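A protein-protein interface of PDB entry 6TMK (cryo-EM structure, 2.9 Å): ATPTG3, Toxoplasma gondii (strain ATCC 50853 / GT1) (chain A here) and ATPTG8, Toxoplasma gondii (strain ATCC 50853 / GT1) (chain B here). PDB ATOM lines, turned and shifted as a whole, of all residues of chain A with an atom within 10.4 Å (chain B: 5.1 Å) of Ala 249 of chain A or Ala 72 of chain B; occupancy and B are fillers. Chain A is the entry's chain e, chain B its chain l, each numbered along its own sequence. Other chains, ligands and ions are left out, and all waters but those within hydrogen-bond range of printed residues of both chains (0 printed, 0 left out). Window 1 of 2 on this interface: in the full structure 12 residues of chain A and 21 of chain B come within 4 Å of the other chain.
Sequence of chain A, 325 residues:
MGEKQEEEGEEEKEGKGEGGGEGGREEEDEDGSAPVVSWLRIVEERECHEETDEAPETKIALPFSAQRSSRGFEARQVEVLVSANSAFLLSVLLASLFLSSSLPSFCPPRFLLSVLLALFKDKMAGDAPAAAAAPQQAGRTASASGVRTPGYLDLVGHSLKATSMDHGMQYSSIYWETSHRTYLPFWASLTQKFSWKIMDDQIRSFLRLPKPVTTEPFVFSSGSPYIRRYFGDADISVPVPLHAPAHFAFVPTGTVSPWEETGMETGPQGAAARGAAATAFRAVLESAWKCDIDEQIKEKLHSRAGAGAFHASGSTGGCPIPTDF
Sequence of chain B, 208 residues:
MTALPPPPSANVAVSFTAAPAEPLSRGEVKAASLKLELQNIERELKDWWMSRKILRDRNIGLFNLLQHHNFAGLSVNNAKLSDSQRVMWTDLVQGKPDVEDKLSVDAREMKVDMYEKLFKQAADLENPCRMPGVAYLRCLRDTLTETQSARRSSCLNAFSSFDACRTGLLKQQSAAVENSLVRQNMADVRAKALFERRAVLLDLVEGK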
ATOM      1  N   PRO A 245     -14.807  18.481  23.549  1.00  0.00           N
ATOM      2  CA  PRO A 245     -15.600  17.255  23.654  1.00  0.00           C
ATOM      3  C   PRO A 245     -14.733  16.062  24.015  1.00  0.00           C
ATOM      4  O   PRO A 245     -13.648  15.872  23.465  1.00  0.00           O
ATOM      5  CB  PRO A 245     -16.209  17.112  22.257  1.00  0.00           C
ATOM      6  CG  PRO A 245     -15.227  17.757  21.378  1.00  0.00           C
ATOM      7  CD  PRO A 245     -14.689  18.923  22.151  1.00  0.00           C
ATOM      8  N   ALA A 246     -15.216  15.268  24.962  1.00  0.00           N
ATOM      9  CA  ALA A 246     -14.571  14.013  25.293  1.00  0.00           C
ATOM     10  C   ALA A 246     -15.059  12.933  24.345  1.00  0.00           C
ATOM     11  O   ALA A 246     -16.259  12.824  24.074  1.00  0.00           O
ATOM     12  CB  ALA A 246     -14.860  13.620  26.737  1.00  0.00           C
ATOM     13  N   HIS A 247     -14.129  12.145  23.831  1.00  0.00           N
ATOM     14  CA  HIS A 247     -14.438  11.054  22.930  1.00  0.00           C
ATOM     15  C   HIS A 247     -14.108   9.732  23.603  1.00  0.00           C
ATOM     16  O   HIS A 247     -13.325   9.671  24.554  1.00  0.00           O
ATOM     17  CB  HIS A 247     -13.676  11.210  21.617  1.00  0.00           C
ATOM     18  CG  HIS A 247     -13.880  12.537  20.960  1.00  0.00           C
ATOM     19  ND1 HIS A 247     -12.911  13.514  20.940  1.00  0.00           N
ATOM     20  CD2 HIS A 247     -14.946  13.052  20.306  1.00  0.00           C
ATOM     21  CE1 HIS A 247     -13.369  14.574  20.301  1.00  0.00           C
ATOM     22  NE2 HIS A 247     -14.602  14.319  19.905  1.00  0.00           N
ATOM     23  N   PHE A 248     -14.732   8.671  23.109  1.00  0.00           N
ATOM     24  CA  PHE A 248     -14.691   7.381  23.769  1.00  0.00           C
ATOM     25  C   PHE A 248     -14.555   6.284  22.729  1.00  0.00           C
ATOM     26  O   PHE A 248     -15.041   6.407  21.604  1.00  0.00           O
ATOM     27  CB  PHE A 248     -15.943   7.148  24.616  1.00  0.00           C
ATOM     28  CG  PHE A 248     -16.145   8.168  25.692  1.00  0.00           C
ATOM     29  CD1 PHE A 248     -16.848   9.326  25.441  1.00  0.00           C
ATOM     30  CD2 PHE A 248     -15.633   7.971  26.956  1.00  0.00           C
ATOM     31  CE1 PHE A 248     -17.035  10.258  26.424  1.00  0.00           C
ATOM     32  CE2 PHE A 248     -15.818   8.904  27.939  1.00  0.00           C
ATOM     33  CZ  PHE A 248     -16.517  10.047  27.673  1.00  0.00           C
ATOM     34  N   ALA A 249     -13.884   5.206  23.124  1.00  0.00           N
ATOM     35  CA  ALA A 249     -13.604   4.083  22.242  1.00  0.00           C
ATOM     36  C   ALA A 249     -13.808   2.797  23.020  1.00  0.00           C
ATOM     37  O   ALA A 249     -13.073   2.523  23.972  1.00  0.00           O
ATOM     38  CB  ALA A 249     -12.185   4.155  21.681  1.00  0.00           C
ATOM     39  N   PHE A 250     -14.796   2.010  22.609  1.00  0.00           N
ATOM     40  CA  PHE A 250     -15.069   0.715  23.226  1.00  0.00           C
ATOM     41  C   PHE A 250     -14.235  -0.367  22.543  1.00  0.00           C
ATOM     42  O   PHE A 250     -14.732  -1.362  22.022  1.00  0.00           O
ATOM     43  CB  PHE A 250     -16.561   0.413  23.149  1.00  0.00           C
ATOM     44  CG  PHE A 250     -17.074  -0.438  24.263  1.00  0.00           C
ATOM     45  CD1 PHE A 250     -17.338   0.109  25.500  1.00  0.00           C
ATOM     46  CD2 PHE A 250     -17.313  -1.779  24.073  1.00  0.00           C
ATOM     47  CE1 PHE A 250     -17.813  -0.667  26.521  1.00  0.00           C
ATOM     48  CE2 PHE A 250     -17.791  -2.557  25.095  1.00  0.00           C
ATOM     49  CZ  PHE A 250     -18.042  -1.998  26.319  1.00  0.00           C
ATOM     50  N   VAL A 251     -12.927  -0.136  22.562  1.00  0.00           N
ATOM     51  CA  VAL A 251     -11.978  -0.905  21.765  1.00  0.00           C
ATOM     52  C   VAL A 251     -10.827  -1.342  22.658  1.00  0.00           C
ATOM     53  O   VAL A 251     -10.387  -0.566  23.517  1.00  0.00           O
ATOM     54  CB  VAL A 251     -11.459  -0.089  20.573  1.00  0.00           C
ATOM     55  CG1 VAL A 251     -10.507  -0.905  19.762  1.00  0.00           C
ATOM     56  CG2 VAL A 251     -12.585   0.365  19.711  1.00  0.00           C
ATOM     57  N   PRO A 252     -10.305  -2.554  22.498  1.00  0.00           N
ATOM     58  CA  PRO A 252      -9.067  -2.920  23.182  1.00  0.00           C
ATOM     59  C   PRO A 252      -7.823  -2.585  22.378  1.00  0.00           C
ATOM     60  O   PRO A 252      -7.803  -2.631  21.148  1.00  0.00           O
ATOM     61  CB  PRO A 252      -9.220  -4.436  23.347  1.00  0.00           C
ATOM     62  CG  PRO A 252      -9.972  -4.834  22.164  1.00  0.00           C
ATOM     63  CD  PRO A 252     -10.947  -3.733  21.897  1.00  0.00           C
ATOM     64  N   THR A 253      -6.768  -2.249  23.107  1.00  0.00           N
ATOM     65  CA  THR A 253      -5.514  -1.830  22.507  1.00  0.00           C
ATOM     66  C   THR A 253      -4.619  -3.026  22.215  1.00  0.00           C
ATOM     67  O   THR A 253      -4.623  -4.024  22.938  1.00  0.00           O
ATOM     68  CB  THR A 253      -4.779  -0.855  23.422  1.00  0.00           C
ATOM     69  OG1 THR A 253      -4.627  -1.429  24.724  1.00  0.00           O
ATOM     70  CG2 THR A 253      -5.538   0.430  23.535  1.00  0.00           C
ATOM     71  N   ASN B  70      -8.715  14.130  23.458  1.00  0.00           N
ATOM     72  CA  ASN B  70      -9.398  13.807  24.708  1.00  0.00           C
ATOM     73  C   ASN B  70     -10.220  12.522  24.583  1.00  0.00           C
ATOM     74  O   ASN B  70     -11.445  12.518  24.703  1.00  0.00           O
ATOM     75  CB  ASN B  70     -10.263  14.980  25.169  1.00  0.00           C
ATOM     76  CG  ASN B  70     -10.663  14.871  26.618  1.00  0.00           C
ATOM     77  OD1 ASN B  70     -10.015  14.187  27.406  1.00  0.00           O
ATOM     78  ND2 ASN B  70     -11.726  15.561  26.983  1.00  0.00           N
ATOM     79  N   PHE B  71      -9.517  11.424  24.342  1.00  0.00           N
ATOM     80  CA  PHE B  71     -10.122  10.107  24.237  1.00  0.00           C
ATOM     81  C   PHE B  71     -10.009   9.346  25.547  1.00  0.00           C
ATOM     82  O   PHE B  71      -9.113   9.588  26.360  1.00  0.00           O
ATOM     83  CB  PHE B  71      -9.485   9.282  23.121  1.00  0.00           C
ATOM     84  CG  PHE B  71     -10.082   9.515  21.775  1.00  0.00           C
ATOM     85  CD1 PHE B  71     -11.027   8.642  21.276  1.00  0.00           C
ATOM     86  CD2 PHE B  71      -9.719  10.599  21.013  1.00  0.00           C
ATOM     87  CE1 PHE B  71     -11.585   8.841  20.048  1.00  0.00           C
ATOM     88  CE2 PHE B  71     -10.278  10.804  19.780  1.00  0.00           C
ATOM     89  CZ  PHE B  71     -11.214   9.926  19.298  1.00  0.00           C
ATOM     90  N   ALA B  72     -10.933   8.411  25.736  1.00  0.00           N
ATOM     91  CA  ALA B  72     -10.936   7.527  26.888  1.00  0.00           C
ATOM     92  C   ALA B  72     -11.310   6.134  26.417  1.00  0.00           C
ATOM     93  O   ALA B  72     -12.252   5.971  25.636  1.00  0.00           O
ATOM     94  CB  ALA B  72     -11.916   8.011  27.957  1.00  0.00           C
ATOM     95  N   GLY B  73     -10.569   5.140  26.889  1.00  0.00           N
ATOM     96  CA  GLY B  73     -10.779   3.768  26.487  1.00  0.00           C
ATOM     97  C   GLY B  73     -11.233   2.871  27.614  1.00  0.00           C
ATOM     98  O   GLY B  73     -11.713   3.343  28.647  1.00  0.00           O
ATOM     99  N   LEU B  74     -11.072   1.563  27.423  1.00  0.00           N
ATOM    100  CA  LEU B  74     -11.479   0.611  28.448  1.00  0.00           C
ATOM    101  C   LEU B  74     -10.661   0.795  29.716  1.00  0.00           C
ATOM    102  O   LEU B  74     -11.171   0.619  30.826  1.00  0.00           O
ATOM    103  CB  LEU B  74     -11.330  -0.809  27.919  1.00  0.00           C
ATOM    104  CG  LEU B  74     -11.987  -1.115  26.578  1.00  0.00           C
ATOM    105  CD1 LEU B  74     -11.686  -2.530  26.176  1.00  0.00           C
ATOM    106  CD2 LEU B  74     -13.469  -0.886  26.619  1.00  0.00           C
ATOM    107  N   ASN B  78      -7.791   9.005  31.799  1.00  0.00           N
ATOM    108  CA  ASN B  78      -7.951  10.379  31.351  1.00  0.00           C
ATOM    109  C   ASN B  78      -8.356  11.237  32.536  1.00  0.00           C
ATOM    110  O   ASN B  78      -9.340  10.936  33.220  1.00  0.00           O
ATOM    111  CB  ASN B  78      -8.989  10.471  30.236  1.00  0.00           C
ATOM    112  CG  ASN B  78      -9.031  11.835  29.598  1.00  0.00           C
ATOM    113  OD1 ASN B  78      -8.195  12.691  29.880  1.00  0.00           O
ATOM    114  ND2 ASN B  78      -9.998  12.044  28.721  1.00  0.00           N
ATOM    115  N   LEU B  81     -11.540  14.317  32.131  1.00  0.00           N
ATOM    116  CA  LEU B  81     -12.941  13.947  32.028  1.00  0.00           C
ATOM    117  C   LEU B  81     -13.780  14.658  33.081  1.00  0.00           C
ATOM    118  O   LEU B  81     -13.312  14.977  34.177  1.00  0.00           O
ATOM    119  CB  LEU B  81     -13.114  12.442  32.201  1.00  0.00           C
ATOM    120  CG  LEU B  81     -12.930  11.535  30.995  1.00  0.00           C
ATOM    121  CD1 LEU B  81     -13.099  10.100  31.421  1.00  0.00           C
ATOM    122  CD2 LEU B  81     -13.931  11.886  29.941  1.00  0.00           C
ATOM    123  N   TRP B  89     -19.147   6.262  31.667  1.00  0.00           N
ATOM    124  CA  TRP B  89     -18.240   5.374  30.955  1.00  0.00           C
ATOM    125  C   TRP B  89     -17.850   4.175  31.811  1.00  0.00           C
ATOM    126  O   TRP B  89     -17.768   3.047  31.310  1.00  0.00           O
ATOM    127  CB  TRP B  89     -17.014   6.165  30.517  1.00  0.00           C
ATOM    128  CG  TRP B  89     -16.090   5.431  29.630  1.00  0.00           C
ATOM    129  CD1 TRP B  89     -14.781   5.162  29.860  1.00  0.00           C
ATOM    130  CD2 TRP B  89     -16.399   4.871  28.356  1.00  0.00           C
ATOM    131  NE1 TRP B  89     -14.251   4.467  28.811  1.00  0.00           N
ATOM    132  CE2 TRP B  89     -15.227   4.274  27.871  1.00  0.00           C
ATOM    133  CE3 TRP B  89     -17.553   4.814  27.577  1.00  0.00           C
ATOM    134  CZ2 TRP B  89     -15.177   3.630  26.648  1.00  0.00           C
ATOM    135  CZ3 TRP B  89     -17.496   4.178  26.368  1.00  0.00           C
ATOM    136  CH2 TRP B  89     -16.320   3.594  25.915  1.00  0.00           C
ATOM    137  N   ALA B 122     -19.052   5.330  20.597  1.00  0.00           N
ATOM    138  CA  ALA B 122     -17.881   4.568  21.006  1.00  0.00           C
ATOM    139  C   ALA B 122     -17.718   3.298  20.185  1.00  0.00           C
ATOM    140  O   ALA B 122     -16.621   3.000  19.704  1.00  0.00           O
ATOM    141  CB  ALA B 122     -17.976   4.231  22.489  1.00  0.00           C
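Pro 245 of chain A touches Asn 70 of chain B (O to CB, 3.9 Å).
Ala 246 of chain A touches Asn 70 of chain B (CA to O, 3.5 Å).
O of His 247 of chain A touches CA of Phe 71 of chain B, at 3.2 Å.
Ala 72 of chain B touches Phe 248 of chain A (O to CA, 3.4 Å).
Phe 248 of chain A touches Leu 81 of chain B.
Phe 248 of chain A touches Ala 122 of chain B (O to CA, 3.4 Å).
Ala 249 of chain A touches Trp 89 of chain B.
Ala 122 of chain B touches Phe 250 of chain A.
CG of Leu 74 of chain B touches O of Val 251 of chain A (3.5 Å).
Pro 252 of chain A touches Leu 74 of chain B (N to CD1, 3.9 Å).
The side-chain amide oxygen of Asn 70 of chain B lies within hydrogen-bond range of the side-chain amide nitrogen of Asn 78 of chain B (2.5 Å).
The indole nitrogen (NE1) of Trp 89 of chain B is in hydrogen-bond range of the backbone carbonyl oxygen (O) of Gly 73 of chain B (2.8 Å).
The backbone NH (N) of His 247 of chain A is in hydrogen-bond range of the backbone carbonyl oxygen (O) of Asn 70 of chain B (2.8 Å).
The backbone carbonyl oxygen (O) of His 247 of chain A sits at hydrogen-bond distance from the backbone NH (N) of Ala 72 of chain B.
O of Ala 72 of chain B lies within hydrogen-bond range of N of Ala 249 of chain A (3.1 Å).
Of the 9 printed residues of chain B, 8 touch a printed residue of chain A.
Hydrophobic or aromatic side chains of chain B that line the printed part of chain A: Phe 71, Ala 72, Leu 74, Leu 81, Trp 89 and Ala 122.
Along chain B the printed residues that touch a printed residue of chain A span positions 70 to 122.
Ala 249 of chain A touches just these residues of chain B: Ala 72 (3.1 Å), Gly 73 (3.6 Å) and Trp 89 (3.6 Å).
Of chain A, only His 247, Phe 248 and Ala 249 come within 4 Å of Ala 72 of chain B.
Printed residues of chain A within 4 Å of Trp 89 of chain B: Phe 248, Ala 249 and Phe 250.
Of the printed residues of chain B, Ala 246 of chain A touches Asn 70 and Leu 81.
Of the printed residues of chain B, Pro 245 of chain A touches Asn 70 (3.9 Å).
Printed residues of chain B within 4 Å of His 247 of chain A: Asn 70, Phe 71 and Ala 72.
The nearest printed residue of chain B that does not touch Ala 249 of chain A is Ala 122 of chain B (4.1 Å).
The nearest printed residue of chain B that does not touch Phe 250 of chain A is Leu 74 of chain B (4.1 Å).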
